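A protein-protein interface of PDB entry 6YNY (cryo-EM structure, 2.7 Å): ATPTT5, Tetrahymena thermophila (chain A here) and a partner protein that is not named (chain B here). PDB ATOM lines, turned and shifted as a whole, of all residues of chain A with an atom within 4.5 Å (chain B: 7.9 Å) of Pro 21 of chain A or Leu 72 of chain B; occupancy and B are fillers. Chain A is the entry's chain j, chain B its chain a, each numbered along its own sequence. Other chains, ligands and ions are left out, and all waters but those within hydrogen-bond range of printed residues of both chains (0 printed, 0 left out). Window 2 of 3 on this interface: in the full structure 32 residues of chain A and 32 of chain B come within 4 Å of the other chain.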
ATOM      1  N   ILE A  10      13.825 -19.731 -17.314  1.00  0.00           N
ATOM      2  CA  ILE A  10      15.031 -19.929 -16.521  1.00  0.00           C
ATOM      3  C   ILE A  10      16.212 -19.252 -17.199  1.00  0.00           C
ATOM      4  O   ILE A  10      16.121 -18.818 -18.352  1.00  0.00           O
ATOM      5  CB  ILE A  10      15.311 -21.420 -16.280  1.00  0.00           C
ATOM      6  CG1 ILE A  10      15.576 -22.150 -17.592  1.00  0.00           C
ATOM      7  CG2 ILE A  10      14.150 -22.044 -15.562  1.00  0.00           C
ATOM      8  CD1 ILE A  10      16.046 -23.547 -17.396  1.00  0.00           C
ATOM      9  N   ALA A  12      18.866 -20.471 -18.377  1.00  0.00           N
ATOM     10  CA  ALA A  12      19.396 -21.182 -19.534  1.00  0.00           C
ATOM     11  C   ALA A  12      18.714 -20.752 -20.824  1.00  0.00           C
ATOM     12  O   ALA A  12      19.316 -20.844 -21.899  1.00  0.00           O
ATOM     13  CB  ALA A  12      19.245 -22.686 -19.337  1.00  0.00           C
ATOM     14  N   HIS A  16      20.605 -19.769 -24.753  1.00  0.00           N
ATOM     15  CA  HIS A  16      20.336 -20.339 -26.063  1.00  0.00           C
ATOM     16  C   HIS A  16      19.277 -19.570 -26.834  1.00  0.00           C
ATOM     17  O   HIS A  16      19.268 -19.613 -28.068  1.00  0.00           O
ATOM     18  CB  HIS A  16      19.889 -21.792 -25.912  1.00  0.00           C
ATOM     19  CG  HIS A  16      20.784 -22.609 -25.038  1.00  0.00           C
ATOM     20  ND1 HIS A  16      21.911 -23.244 -25.511  1.00  0.00           N
ATOM     21  CD2 HIS A  16      20.719 -22.890 -23.716  1.00  0.00           C
ATOM     22  CE1 HIS A  16      22.501 -23.882 -24.517  1.00  0.00           C
ATOM     23  NE2 HIS A  16      21.798 -23.684 -23.417  1.00  0.00           N
ATOM     24  N   THR A  18      16.236 -20.220 -27.141  1.00  0.00           N
ATOM     25  CA  THR A  18      15.228 -21.101 -27.706  1.00  0.00           C
ATOM     26  C   THR A  18      14.980 -22.249 -26.743  1.00  0.00           C
ATOM     27  O   THR A  18      15.856 -22.623 -25.960  1.00  0.00           O
ATOM     28  CB  THR A  18      15.655 -21.652 -29.069  1.00  0.00           C
ATOM     29  OG1 THR A  18      14.596 -22.441 -29.621  1.00  0.00           O
ATOM     30  CG2 THR A  18      16.887 -22.515 -28.932  1.00  0.00           C
ATOM     31  N   HIS A  19      13.774 -22.802 -26.809  1.00  0.00           N
ATOM     32  CA  HIS A  19      13.428 -23.987 -26.041  1.00  0.00           C
ATOM     33  C   HIS A  19      13.758 -25.279 -26.769  1.00  0.00           C
ATOM     34  O   HIS A  19      13.721 -26.347 -26.149  1.00  0.00           O
ATOM     35  CB  HIS A  19      11.938 -23.997 -25.699  1.00  0.00           C
ATOM     36  CG  HIS A  19      11.507 -22.871 -24.814  1.00  0.00           C
ATOM     37  ND1 HIS A  19      10.716 -21.836 -25.263  1.00  0.00           N
ATOM     38  CD2 HIS A  19      11.743 -22.623 -23.506  1.00  0.00           C
ATOM     39  CE1 HIS A  19      10.488 -20.997 -24.269  1.00  0.00           C
ATOM     40  NE2 HIS A  19      11.103 -21.451 -23.193  1.00  0.00           N
ATOM     41  N   TYR A  20      14.090 -25.211 -28.057  1.00  0.00           N
ATOM     42  CA  TYR A  20      14.267 -26.392 -28.898  1.00  0.00           C
ATOM     43  C   TYR A  20      15.678 -26.469 -29.473  1.00  0.00           C
ATOM     44  O   TYR A  20      15.860 -26.501 -30.695  1.00  0.00           O
ATOM     45  CB  TYR A  20      13.235 -26.389 -30.020  1.00  0.00           C
ATOM     46  CG  TYR A  20      11.814 -26.258 -29.543  1.00  0.00           C
ATOM     47  CD1 TYR A  20      11.057 -27.375 -29.247  1.00  0.00           C
ATOM     48  CD2 TYR A  20      11.228 -25.015 -29.390  1.00  0.00           C
ATOM     49  CE1 TYR A  20       9.761 -27.259 -28.811  1.00  0.00           C
ATOM     50  CE2 TYR A  20       9.931 -24.890 -28.954  1.00  0.00           C
ATOM     51  CZ  TYR A  20       9.201 -26.016 -28.666  1.00  0.00           C
ATOM     52  OH  TYR A  20       7.904 -25.901 -28.230  1.00  0.00           O
ATOM     53  N   PRO A  21      16.702 -26.494 -28.623  1.00  0.00           N
ATOM     54  CA  PRO A  21      18.050 -26.830 -29.093  1.00  0.00           C
ATOM     55  C   PRO A  21      18.206 -28.338 -29.181  1.00  0.00           C
ATOM     56  O   PRO A  21      18.277 -29.030 -28.162  1.00  0.00           O
ATOM     57  CB  PRO A  21      18.948 -26.226 -28.008  1.00  0.00           C
ATOM     58  CG  PRO A  21      18.147 -26.374 -26.793  1.00  0.00           C
ATOM     59  CD  PRO A  21      16.713 -26.154 -27.192  1.00  0.00           C
ATOM     60  N   TYR A  22      18.263 -28.853 -30.401  1.00  0.00           N
ATOM     61  CA  TYR A  22      18.324 -30.295 -30.618  1.00  0.00           C
ATOM     62  C   TYR A  22      19.742 -30.761 -30.333  1.00  0.00           C
ATOM     63  O   TYR A  22      20.580 -30.879 -31.227  1.00  0.00           O
ATOM     64  CB  TYR A  22      17.875 -30.643 -32.026  1.00  0.00           C
ATOM     65  CG  TYR A  22      16.378 -30.692 -32.167  1.00  0.00           C
ATOM     66  CD1 TYR A  22      15.621 -29.534 -32.129  1.00  0.00           C
ATOM     67  CD2 TYR A  22      15.720 -31.895 -32.333  1.00  0.00           C
ATOM     68  CE1 TYR A  22      14.256 -29.576 -32.252  1.00  0.00           C
ATOM     69  CE2 TYR A  22      14.359 -31.946 -32.458  1.00  0.00           C
ATOM     70  CZ  TYR A  22      13.633 -30.784 -32.418  1.00  0.00           C
ATOM     71  OH  TYR A  22      12.272 -30.840 -32.544  1.00  0.00           O
ATOM     72  N   VAL A  23      20.007 -31.030 -29.061  1.00  0.00           N
ATOM     73  CA  VAL A  23      21.320 -31.441 -28.593  1.00  0.00           C
ATOM     74  C   VAL A  23      21.335 -32.958 -28.501  1.00  0.00           C
ATOM     75  O   VAL A  23      20.685 -33.547 -27.631  1.00  0.00           O
ATOM     76  CB  VAL A  23      21.659 -30.801 -27.242  1.00  0.00           C
ATOM     77  CG1 VAL A  23      22.986 -31.305 -26.743  1.00  0.00           C
ATOM     78  CG2 VAL A  23      21.673 -29.300 -27.364  1.00  0.00           C
ATOM     79  N   GLN A  51      14.003 -29.185 -24.812  1.00  0.00           N
ATOM     80  CA  GLN A  51      15.090 -29.622 -23.956  1.00  0.00           C
ATOM     81  C   GLN A  51      15.488 -28.554 -22.952  1.00  0.00           C
ATOM     82  O   GLN A  51      16.363 -28.804 -22.114  1.00  0.00           O
ATOM     83  CB  GLN A  51      16.302 -30.031 -24.799  1.00  0.00           C
ATOM     84  CG  GLN A  51      16.134 -31.377 -25.464  1.00  0.00           C
ATOM     85  CD  GLN A  51      17.315 -31.776 -26.307  1.00  0.00           C
ATOM     86  OE1 GLN A  51      17.522 -31.249 -27.393  1.00  0.00           O
ATOM     87  NE2 GLN A  51      18.091 -32.725 -25.816  1.00  0.00           N
ATOM     88  N   VAL A  52      14.873 -27.383 -23.010  1.00  0.00           N
ATOM     89  CA  VAL A  52      15.051 -26.313 -22.035  1.00  0.00           C
ATOM     90  C   VAL A  52      13.746 -26.173 -21.260  1.00  0.00           C
ATOM     91  O   VAL A  52      12.720 -25.813 -21.853  1.00  0.00           O
ATOM     92  CB  VAL A  52      15.432 -24.987 -22.709  1.00  0.00           C
ATOM     93  CG1 VAL A  52      15.623 -23.913 -21.674  1.00  0.00           C
ATOM     94  CG2 VAL A  52      16.682 -25.154 -23.547  1.00  0.00           C
ATOM     95  N   PRO A  53      13.723 -26.444 -19.959  1.00  0.00           N
ATOM     96  CA  PRO A  53      12.465 -26.372 -19.216  1.00  0.00           C
ATOM     97  C   PRO A  53      12.038 -24.936 -18.959  1.00  0.00           C
ATOM     98  O   PRO A  53      12.789 -23.977 -19.141  1.00  0.00           O
ATOM     99  CB  PRO A  53      12.783 -27.101 -17.914  1.00  0.00           C
ATOM    100  CG  PRO A  53      14.227 -26.927 -17.741  1.00  0.00           C
ATOM    101  CD  PRO A  53      14.828 -26.905 -19.103  1.00  0.00           C
ATOM    102  N   LEU A  62      19.104 -34.651 -22.393  1.00  0.00           N
ATOM    103  CA  LEU A  62      19.946 -34.792 -23.569  1.00  0.00           C
ATOM    104  C   LEU A  62      19.637 -36.100 -24.282  1.00  0.00           C
ATOM    105  O   LEU A  62      19.384 -37.127 -23.647  1.00  0.00           O
ATOM    106  CB  LEU A  62      21.418 -34.738 -23.181  1.00  0.00           C
ATOM    107  CG  LEU A  62      21.857 -33.510 -22.391  1.00  0.00           C
ATOM    108  CD1 LEU A  62      23.307 -33.633 -22.022  1.00  0.00           C
ATOM    109  CD2 LEU A  62      21.623 -32.247 -23.182  1.00  0.00           C
ATOM    110  N   VAL B  69      26.437 -31.409 -16.192  1.00  0.00           N
ATOM    111  CA  VAL B  69      27.180 -31.139 -17.413  1.00  0.00           C
ATOM    112  C   VAL B  69      26.282 -30.631 -18.532  1.00  0.00           C
ATOM    113  O   VAL B  69      26.724 -30.531 -19.676  1.00  0.00           O
ATOM    114  CB  VAL B  69      27.960 -32.387 -17.872  1.00  0.00           C
ATOM    115  CG1 VAL B  69      28.835 -32.898 -16.753  1.00  0.00           C
ATOM    116  CG2 VAL B  69      27.015 -33.468 -18.339  1.00  0.00           C
ATOM    117  N   SER B  70      25.030 -30.306 -18.231  1.00  0.00           N
ATOM    118  CA  SER B  70      24.082 -29.815 -19.222  1.00  0.00           C
ATOM    119  C   SER B  70      23.733 -28.370 -18.909  1.00  0.00           C
ATOM    120  O   SER B  70      23.176 -28.079 -17.845  1.00  0.00           O
ATOM    121  CB  SER B  70      22.822 -30.674 -19.240  1.00  0.00           C
ATOM    122  OG  SER B  70      21.873 -30.175 -20.159  1.00  0.00           O
ATOM    123  N   ASN B  71      24.054 -27.472 -19.836  1.00  0.00           N
ATOM    124  CA  ASN B  71      23.709 -26.065 -19.704  1.00  0.00           C
ATOM    125  C   ASN B  71      22.268 -25.770 -20.094  1.00  0.00           C
ATOM    126  O   ASN B  71      21.866 -24.603 -20.070  1.00  0.00           O
ATOM    127  CB  ASN B  71      24.651 -25.212 -20.554  1.00  0.00           C
ATOM    128  CG  ASN B  71      24.612 -25.580 -22.024  1.00  0.00           C
ATOM    129  OD1 ASN B  71      23.708 -26.277 -22.483  1.00  0.00           O
ATOM    130  ND2 ASN B  71      25.600 -25.115 -22.770  1.00  0.00           N
ATOM    131  N   LEU B  72      21.489 -26.787 -20.449  1.00  0.00           N
ATOM    132  CA  LEU B  72      20.105 -26.588 -20.849  1.00  0.00           C
ATOM    133  C   LEU B  72      19.146 -26.545 -19.673  1.00  0.00           C
ATOM    134  O   LEU B  72      18.052 -25.986 -19.805  1.00  0.00           O
ATOM    135  CB  LEU B  72      19.664 -27.703 -21.797  1.00  0.00           C
ATOM    136  CG  LEU B  72      20.562 -28.019 -22.991  1.00  0.00           C
ATOM    137  CD1 LEU B  72      19.950 -29.123 -23.813  1.00  0.00           C
ATOM    138  CD2 LEU B  72      20.790 -26.802 -23.848  1.00  0.00           C
ATOM    139  N   ASP B  73      19.519 -27.121 -18.540  1.00  0.00           N
ATOM    140  CA  ASP B  73      18.661 -27.214 -17.371  1.00  0.00           C
ATOM    141  C   ASP B  73      19.324 -26.518 -16.188  1.00  0.00           C
ATOM    142  O   ASP B  73      20.410 -25.946 -16.300  1.00  0.00           O
ATOM    143  CB  ASP B  73      18.347 -28.677 -17.048  1.00  0.00           C
ATOM    144  CG  ASP B  73      19.586 -29.489 -16.741  1.00  0.00           C
ATOM    145  OD1 ASP B  73      20.703 -28.944 -16.858  1.00  0.00           O
ATOM    146  OD2 ASP B  73      19.442 -30.675 -16.380  1.00  0.00           O
ATOM    147  N   GLU B  74      18.654 -26.574 -15.041  1.00  0.00           N
ATOM    148  CA  GLU B  74      19.110 -25.897 -13.837  1.00  0.00           C
ATOM    149  C   GLU B  74      20.097 -26.718 -13.017  1.00  0.00           C
ATOM    150  O   GLU B  74      20.504 -26.270 -11.942  1.00  0.00           O
ATOM    151  CB  GLU B  74      17.914 -25.523 -12.962  1.00  0.00           C
ATOM    152  CG  GLU B  74      16.934 -24.580 -13.619  1.00  0.00           C
ATOM    153  CD  GLU B  74      15.905 -24.037 -12.650  1.00  0.00           C
ATOM    154  OE1 GLU B  74      16.254 -23.820 -11.473  1.00  0.00           O
ATOM    155  OE2 GLU B  74      14.745 -23.835 -13.060  1.00  0.00           O
ATOM    156  N   SER B  75      20.489 -27.903 -13.486  1.00  0.00           N
ATOM    157  CA  SER B  75      21.480 -28.699 -12.774  1.00  0.00           C
ATOM    158  C   SER B  75      22.902 -28.216 -13.016  1.00  0.00           C
ATOM    159  O   SER B  75      23.821 -28.685 -12.338  1.00  0.00           O
ATOM    160  CB  SER B  75      21.375 -30.172 -13.177  1.00  0.00           C
ATOM    161  OG  SER B  75      21.834 -30.376 -14.502  1.00  0.00           O
ATOM    162  N   PHE B  76      23.102 -27.301 -13.958  1.00  0.00           N
ATOM    163  CA  PHE B  76      24.432 -26.791 -14.257  1.00  0.00           C
ATOM    164  C   PHE B  76      24.917 -25.905 -13.119  1.00  0.00           C
ATOM    165  O   PHE B  76      24.296 -24.883 -12.811  1.00  0.00           O
ATOM    166  CB  PHE B  76      24.404 -26.015 -15.569  1.00  0.00           C
ATOM    167  CG  PHE B  76      25.758 -25.662 -16.094  1.00  0.00           C
ATOM    168  CD1 PHE B  76      26.541 -26.613 -16.720  1.00  0.00           C
ATOM    169  CD2 PHE B  76      26.244 -24.377 -15.978  1.00  0.00           C
ATOM    170  CE1 PHE B  76      27.781 -26.290 -17.208  1.00  0.00           C
ATOM    171  CE2 PHE B  76      27.488 -24.049 -16.466  1.00  0.00           C
ATOM    172  CZ  PHE B  76      28.255 -25.005 -17.082  1.00  0.00           C
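OE1 of Gln 51 of chain A sits at hydrogen-bond distance from N of Val 23 of chain A (3.0 Å). The backbone carbonyl oxygen of Pro 21 of chain A sits close to the side-chain amide oxygen of Gln 51 of chain A, 2.5 Å away. N of Gln 51 of chain A lies within hydrogen-bond range of O of His 19 of chain A, at 3.1 Å. The side-chain hydroxyl of Ser 70 of chain B lies close to the backbone NH of Leu 72 of chain B, 3.4 Å away.
NE2 of His 16 of chain A lies within hydrogen-bond range of OD1 of Asn 71 of chain B, 3.4 Å away.
Among the printed residues, merely in contact across the chains: Ile 10 of chain A with Glu 74 of chain B, His 16 of chain A with Leu 72 of chain B, Ala 12 of chain A with Asn 71 of chain B, Pro 53 of chain A with Leu 72 of chain B, Gln 51 of chain A with Leu 72 of chain B, Ala 12 of chain A with Leu 72 of chain B, Leu 62 of chain A with Leu 72 of chain B, Leu 62 of chain A with Ser 70 of chain B, Val 52 of chain A with Leu 72 of chain B, Val 23 of chain A with Leu 72 of chain B, Ile 10 of chain A with Leu 72 of chain B and Pro 21 of chain A with Leu 72 of chain B.
Of the 8 printed residues of chain B, 4 touch a printed residue of chain A. Among the printed residues, no Asp or Glu carboxylate lies within 4 Å of a Lys or Arg side-chain nitrogen of the other chain.
Of the printed residues of chain B, Ile 10 of chain A touches Leu 72 (3.97 Å) and Glu 74 (3.1 Å). Printed residues of chain B within 4 Å of His 16 of chain A: Asn 71 (3.4 Å) and Leu 72 (3.3 Å). His 19 of chain A touches none of the printed residues of chain B. Of the printed residues of chain B, Pro 21 of chain A touches Leu 72 (3.98 Å). Printed residues of chain B within 4 Å of Pro 53 of chain A: Leu 72. Printed residues of chain A within 4 Å of Asn 71 of chain B: Ala 12 and His 16. Printed residues of chain A within 4 Å of Leu 72 of chain B: Ile 10 (3.97 Å), Ala 12 (3.5 Å), His 16 (3.3 Å), Pro 21 (3.98 Å), Val 23 (3.95 Å), Gln 51 (3.5 Å), Val 52 (3.7 Å), Pro 53 (3.4 Å) and Leu 62 (3.6 Å). The nearest printed residue of chain B that does not touch Pro 21 of chain A is Asn 71 of chain B (7.0 Å). The nearest printed residue of chain B that does not touch Val 52 of chain A is Asp 73 of chain B (5.7 Å).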
